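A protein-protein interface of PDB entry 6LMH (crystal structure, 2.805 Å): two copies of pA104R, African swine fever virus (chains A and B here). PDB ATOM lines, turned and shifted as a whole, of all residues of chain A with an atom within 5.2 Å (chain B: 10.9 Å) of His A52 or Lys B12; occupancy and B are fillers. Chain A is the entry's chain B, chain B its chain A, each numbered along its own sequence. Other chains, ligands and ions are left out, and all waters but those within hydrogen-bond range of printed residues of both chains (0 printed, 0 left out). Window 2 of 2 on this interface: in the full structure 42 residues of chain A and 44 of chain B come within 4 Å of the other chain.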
ATOM      1  N   ASN A  48     -13.920   6.743 -13.674  1.00  0.00           N
ATOM      2  CA  ASN A  48     -12.804   6.317 -12.839  1.00  0.00           C
ATOM      3  C   ASN A  48     -11.717   5.627 -13.653  1.00  0.00           C
ATOM      4  O   ASN A  48     -10.529   5.768 -13.340  1.00  0.00           O
ATOM      5  CB  ASN A  48     -13.295   5.388 -11.734  1.00  0.00           C
ATOM      6  CG  ASN A  48     -12.189   4.985 -10.792  1.00  0.00           C
ATOM      7  OD1 ASN A  48     -11.626   3.896 -10.905  1.00  0.00           O
ATOM      8  ND2 ASN A  48     -11.851   5.876  -9.866  1.00  0.00           N
ATOM      9  N   ALA A  49     -12.095   4.875 -14.689  1.00  0.00           N
ATOM     10  CA  ALA A  49     -11.095   4.156 -15.467  1.00  0.00           C
ATOM     11  C   ALA A  49     -10.279   5.109 -16.328  1.00  0.00           C
ATOM     12  O   ALA A  49      -9.051   4.992 -16.398  1.00  0.00           O
ATOM     13  CB  ALA A  49     -11.768   3.093 -16.329  1.00  0.00           C
ATOM     14  N   LEU A  50     -10.942   6.058 -16.993  1.00  0.00           N
ATOM     15  CA  LEU A  50     -10.220   7.039 -17.800  1.00  0.00           C
ATOM     16  C   LEU A  50      -9.240   7.840 -16.949  1.00  0.00           C
ATOM     17  O   LEU A  50      -8.118   8.119 -17.383  1.00  0.00           O
ATOM     18  CB  LEU A  50     -11.209   7.967 -18.501  1.00  0.00           C
ATOM     19  CG  LEU A  50     -12.135   7.265 -19.487  1.00  0.00           C
ATOM     20  CD1 LEU A  50     -13.145   8.228 -20.079  1.00  0.00           C
ATOM     21  CD2 LEU A  50     -11.300   6.615 -20.569  1.00  0.00           C
ATOM     22  N   LYS A  51      -9.645   8.210 -15.729  1.00  0.00           N
ATOM     23  CA  LYS A  51      -8.767   8.913 -14.801  1.00  0.00           C
ATOM     24  C   LYS A  51      -7.646   8.032 -14.273  1.00  0.00           C
ATOM     25  O   LYS A  51      -6.770   8.532 -13.559  1.00  0.00           O
ATOM     26  CB  LYS A  51      -9.572   9.476 -13.631  1.00  0.00           C
ATOM     27  CG  LYS A  51     -10.546  10.569 -14.022  1.00  0.00           C
ATOM     28  CD  LYS A  51     -11.291  11.116 -12.811  1.00  0.00           C
ATOM     29  CE  LYS A  51     -11.034  12.606 -12.623  1.00  0.00           C
ATOM     30  NZ  LYS A  51     -12.214  13.326 -12.054  1.00  0.00           N
ATOM     31  N   HIS A  52      -7.662   6.741 -14.593  1.00  0.00           N
ATOM     32  CA  HIS A  52      -6.525   5.857 -14.392  1.00  0.00           C
ATOM     33  C   HIS A  52      -5.891   5.479 -15.728  1.00  0.00           C
ATOM     34  O   HIS A  52      -5.232   4.442 -15.834  1.00  0.00           O
ATOM     35  CB  HIS A  52      -6.951   4.614 -13.604  1.00  0.00           C
ATOM     36  CG  HIS A  52      -7.251   4.885 -12.158  1.00  0.00           C
ATOM     37  ND1 HIS A  52      -7.911   6.018 -11.732  1.00  0.00           N
ATOM     38  CD2 HIS A  52      -6.981   4.166 -11.042  1.00  0.00           C
ATOM     39  CE1 HIS A  52      -8.031   5.988 -10.417  1.00  0.00           C
ATOM     40  NE2 HIS A  52      -7.474   4.875  -9.973  1.00  0.00           N
ATOM     41  N   ASN A  53      -6.092   6.314 -16.751  1.00  0.00           N
ATOM     42  CA  ASN A  53      -5.600   6.081 -18.115  1.00  0.00           C
ATOM     43  C   ASN A  53      -5.872   4.653 -18.580  1.00  0.00           C
ATOM     44  O   ASN A  53      -5.025   3.998 -19.193  1.00  0.00           O
ATOM     45  CB  ASN A  53      -4.117   6.425 -18.249  1.00  0.00           C
ATOM     46  CG  ASN A  53      -3.789   7.032 -19.604  1.00  0.00           C
ATOM     47  OD1 ASN A  53      -3.208   6.378 -20.473  1.00  0.00           O
ATOM     48  ND2 ASN A  53      -4.198   8.280 -19.799  1.00  0.00           N
ATOM     49  N   GLN A  54      -7.073   4.171 -18.277  1.00  0.00           N
ATOM     50  CA  GLN A  54      -7.541   2.855 -18.682  1.00  0.00           C
ATOM     51  C   GLN A  54      -8.671   3.019 -19.693  1.00  0.00           C
ATOM     52  O   GLN A  54      -9.551   3.866 -19.519  1.00  0.00           O
ATOM     53  CB  GLN A  54      -8.018   2.064 -17.460  1.00  0.00           C
ATOM     54  CG  GLN A  54      -8.502   0.655 -17.740  1.00  0.00           C
ATOM     55  CD  GLN A  54      -8.644  -0.179 -16.473  1.00  0.00           C
ATOM     56  OE1 GLN A  54      -8.827   0.358 -15.378  1.00  0.00           O
ATOM     57  NE2 GLN A  54      -8.551  -1.498 -16.617  1.00  0.00           N
ATOM     58  N   GLU A  55      -8.636   2.226 -20.757  1.00  0.00           N
ATOM     59  CA  GLU A  55      -9.656   2.312 -21.794  1.00  0.00           C
ATOM     60  C   GLU A  55     -10.852   1.444 -21.422  1.00  0.00           C
ATOM     61  O   GLU A  55     -10.729   0.477 -20.666  1.00  0.00           O
ATOM     62  CB  GLU A  55      -9.082   1.885 -23.147  1.00  0.00           C
ATOM     63  CG  GLU A  55      -7.744   2.527 -23.453  1.00  0.00           C
ATOM     64  CD  GLU A  55      -7.423   2.561 -24.931  1.00  0.00           C
ATOM     65  OE1 GLU A  55      -8.174   3.208 -25.694  1.00  0.00           O
ATOM     66  OE2 GLU A  55      -6.410   1.950 -25.326  1.00  0.00           O
ATOM     67  N   LYS B  12      -2.363  -0.900 -17.253  1.00  0.00           N
ATOM     68  CA  LYS B  12      -3.747  -1.335 -17.094  1.00  0.00           C
ATOM     69  C   LYS B  12      -4.475  -1.334 -18.436  1.00  0.00           C
ATOM     70  O   LYS B  12      -4.668  -0.286 -19.050  1.00  0.00           O
ATOM     71  CB  LYS B  12      -4.473  -0.446 -16.086  1.00  0.00           C
ATOM     72  CG  LYS B  12      -3.908  -0.552 -14.680  1.00  0.00           C
ATOM     73  CD  LYS B  12      -4.274   0.643 -13.810  1.00  0.00           C
ATOM     74  CE  LYS B  12      -4.153   1.972 -14.546  1.00  0.00           C
ATOM     75  NZ  LYS B  12      -2.968   2.115 -15.452  1.00  0.00           N
ATOM     76  N   PRO B  13      -4.886  -2.515 -18.873  1.00  0.00           N
ATOM     77  CA  PRO B  13      -5.418  -2.687 -20.228  1.00  0.00           C
ATOM     78  C   PRO B  13      -6.887  -2.274 -20.318  1.00  0.00           C
ATOM     79  O   PRO B  13      -7.486  -1.796 -19.360  1.00  0.00           O
ATOM     80  CB  PRO B  13      -5.240  -4.184 -20.467  1.00  0.00           C
ATOM     81  CG  PRO B  13      -5.409  -4.782 -19.092  1.00  0.00           C
ATOM     82  CD  PRO B  13      -4.832  -3.783 -18.124  1.00  0.00           C
ATOM     83  N   THR B  14      -7.461  -2.486 -21.501  1.00  0.00           N
ATOM     84  CA  THR B  14      -8.810  -2.025 -21.797  1.00  0.00           C
ATOM     85  C   THR B  14      -9.853  -2.831 -21.018  1.00  0.00           C
ATOM     86  O   THR B  14      -9.622  -3.974 -20.621  1.00  0.00           O
ATOM     87  CB  THR B  14      -9.059  -2.101 -23.311  1.00  0.00           C
ATOM     88  OG1 THR B  14      -8.172  -1.193 -23.978  1.00  0.00           O
ATOM     89  CG2 THR B  14     -10.491  -1.727 -23.684  1.00  0.00           C
ATOM     90  N   ILE B  15     -11.001  -2.199 -20.777  1.00  0.00           N
ATOM     91  CA  ILE B  15     -12.115  -2.788 -20.044  1.00  0.00           C
ATOM     92  C   ILE B  15     -13.193  -3.146 -21.058  1.00  0.00           C
ATOM     93  O   ILE B  15     -13.769  -2.266 -21.714  1.00  0.00           O
ATOM     94  CB  ILE B  15     -12.648  -1.839 -18.966  1.00  0.00           C
ATOM     95  CG1 ILE B  15     -11.715  -1.848 -17.760  1.00  0.00           C
ATOM     96  CG2 ILE B  15     -14.068  -2.220 -18.556  1.00  0.00           C
ATOM     97  CD1 ILE B  15     -12.233  -1.050 -16.596  1.00  0.00           C
ATOM     98  N   THR B  16     -13.466  -4.438 -21.184  1.00  0.00           N
ATOM     99  CA  THR B  16     -14.391  -4.948 -22.181  1.00  0.00           C
ATOM    100  C   THR B  16     -15.836  -4.720 -21.753  1.00  0.00           C
ATOM    101  O   THR B  16     -16.127  -4.431 -20.592  1.00  0.00           O
ATOM    102  CB  THR B  16     -14.150  -6.436 -22.400  1.00  0.00           C
ATOM    103  OG1 THR B  16     -14.409  -7.140 -21.177  1.00  0.00           O
ATOM    104  CG2 THR B  16     -12.712  -6.664 -22.802  1.00  0.00           C
ATOM    105  N   GLU B  19     -16.658  -7.242 -19.100  1.00  0.00           N
ATOM    106  CA  GLU B  19     -16.158  -6.847 -17.788  1.00  0.00           C
ATOM    107  C   GLU B  19     -16.920  -5.639 -17.256  1.00  0.00           C
ATOM    108  O   GLU B  19     -17.122  -5.520 -16.042  1.00  0.00           O
ATOM    109  CB  GLU B  19     -14.651  -6.568 -17.841  1.00  0.00           C
ATOM    110  CG  GLU B  19     -14.058  -5.888 -16.586  1.00  0.00           C
ATOM    111  CD  GLU B  19     -14.140  -6.721 -15.294  1.00  0.00           C
ATOM    112  OE1 GLU B  19     -15.237  -7.190 -14.919  1.00  0.00           O
ATOM    113  OE2 GLU B  19     -13.093  -6.889 -14.632  1.00  0.00           O
ATOM    114  N   MET B 108     -15.255  14.912 -18.323  1.00  0.00           N
ATOM    115  CA  MET B 108     -15.065  13.687 -17.561  1.00  0.00           C
ATOM    116  C   MET B 108     -13.717  13.645 -16.856  1.00  0.00           C
ATOM    117  O   MET B 108     -13.555  12.884 -15.898  1.00  0.00           O
ATOM    118  CB  MET B 108     -15.208  12.475 -18.481  1.00  0.00           C
ATOM    119  CG  MET B 108     -15.580  11.191 -17.770  1.00  0.00           C
ATOM    120  SD  MET B 108     -16.486  10.066 -18.841  1.00  0.00           S
ATOM    121  CE  MET B 108     -18.170  10.630 -18.633  1.00  0.00           C
ATOM    122  N   LEU B 109     -12.749  14.443 -17.299  1.00  0.00           N
ATOM    123  CA  LEU B 109     -11.452  14.468 -16.639  1.00  0.00           C
ATOM    124  C   LEU B 109     -11.350  15.551 -15.571  1.00  0.00           C
ATOM    125  O   LEU B 109     -10.429  15.502 -14.747  1.00  0.00           O
ATOM    126  CB  LEU B 109     -10.337  14.647 -17.674  1.00  0.00           C
ATOM    127  CG  LEU B 109     -10.102  13.410 -18.550  1.00  0.00           C
ATOM    128  CD1 LEU B 109      -8.915  13.613 -19.472  1.00  0.00           C
ATOM    129  CD2 LEU B 109      -9.912  12.162 -17.699  1.00  0.00           C
ATOM    130  N   ASN B 110     -12.273  16.511 -15.561  1.00  0.00           N
ATOM    131  CA  ASN B 110     -12.326  17.520 -14.513  1.00  0.00           C
ATOM    132  C   ASN B 110     -12.577  16.863 -13.157  1.00  0.00           C
ATOM    133  O   ASN B 110     -13.634  16.269 -12.928  1.00  0.00           O
ATOM    134  CB  ASN B 110     -13.414  18.562 -14.804  1.00  0.00           C
ATOM    135  CG  ASN B 110     -13.370  19.086 -16.238  1.00  0.00           C
ATOM    136  OD1 ASN B 110     -12.417  18.834 -16.983  1.00  0.00           O
ATOM    137  ND2 ASN B 110     -14.399  19.843 -16.620  1.00  0.00           N
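Lys A51 touches Leu B109 (CE to O, 3.6 Å). Gln A54 touches Ile B15 (NE2 to CG1, 3.4 Å). CB of Glu A55 touches OG1 of Thr B14, 3.3 Å away.
Printed residues of chain A that touch a printed residue of chain B: Lys A51, His A52, Gln A54 and Glu A55.
His A52 touches just one residue of chain B: Lys B12 (3.0 Å). Lys B12 touches just one residue of chain A: His A52. Gln A54 touches just these residues of chain B: Pro B13 (3.0 Å) and Ile B15 (3.4 Å). Of the printed residues of chain A, Leu B109 touches Lys A51. Of the printed residues of chain A, Ile B15 touches Gln A54 and Glu A55. Of the printed residues of chain A, Thr B14 touches Glu A55. Printed residues of chain A within 4 Å of Asn B110: Lys A51 (3.4 Å). Thr B16 touches none of the printed residues of chain A. Glu B19 touches none of the printed residues of chain A. The nearest residue of chain B that does not touch His A52 is Leu B109 (6.6 Å). The nearest residue of chain A that does not touch Lys B12 is Gln A54 (4.2 Å).
No position is printed for both chains.
The side-chain amino group (NZ) of Lys B12 sits close to the backbone carbonyl oxygen (O) of His A52. The side-chain amide nitrogen (NE2) of Gln A54 sits at hydrogen-bond distance from the backbone carbonyl oxygen (O) of Pro B13, 3.0 Å away. The backbone NH of Ile B15 is in hydrogen-bond range of the backbone carbonyl oxygen of Glu A55 (2.7 Å). The backbone carbonyl oxygen of Asn B110 lies within hydrogen-bond range of the side-chain amino group of Lys A51, at 3.4 Å.
O of Asn A48 sits at hydrogen-bond distance from ND1 of His A52 (3.1 Å). The backbone carbonyl oxygen of Ala A49 lies within hydrogen-bond range of the backbone NH of Gln A54, at 2.8 Å.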
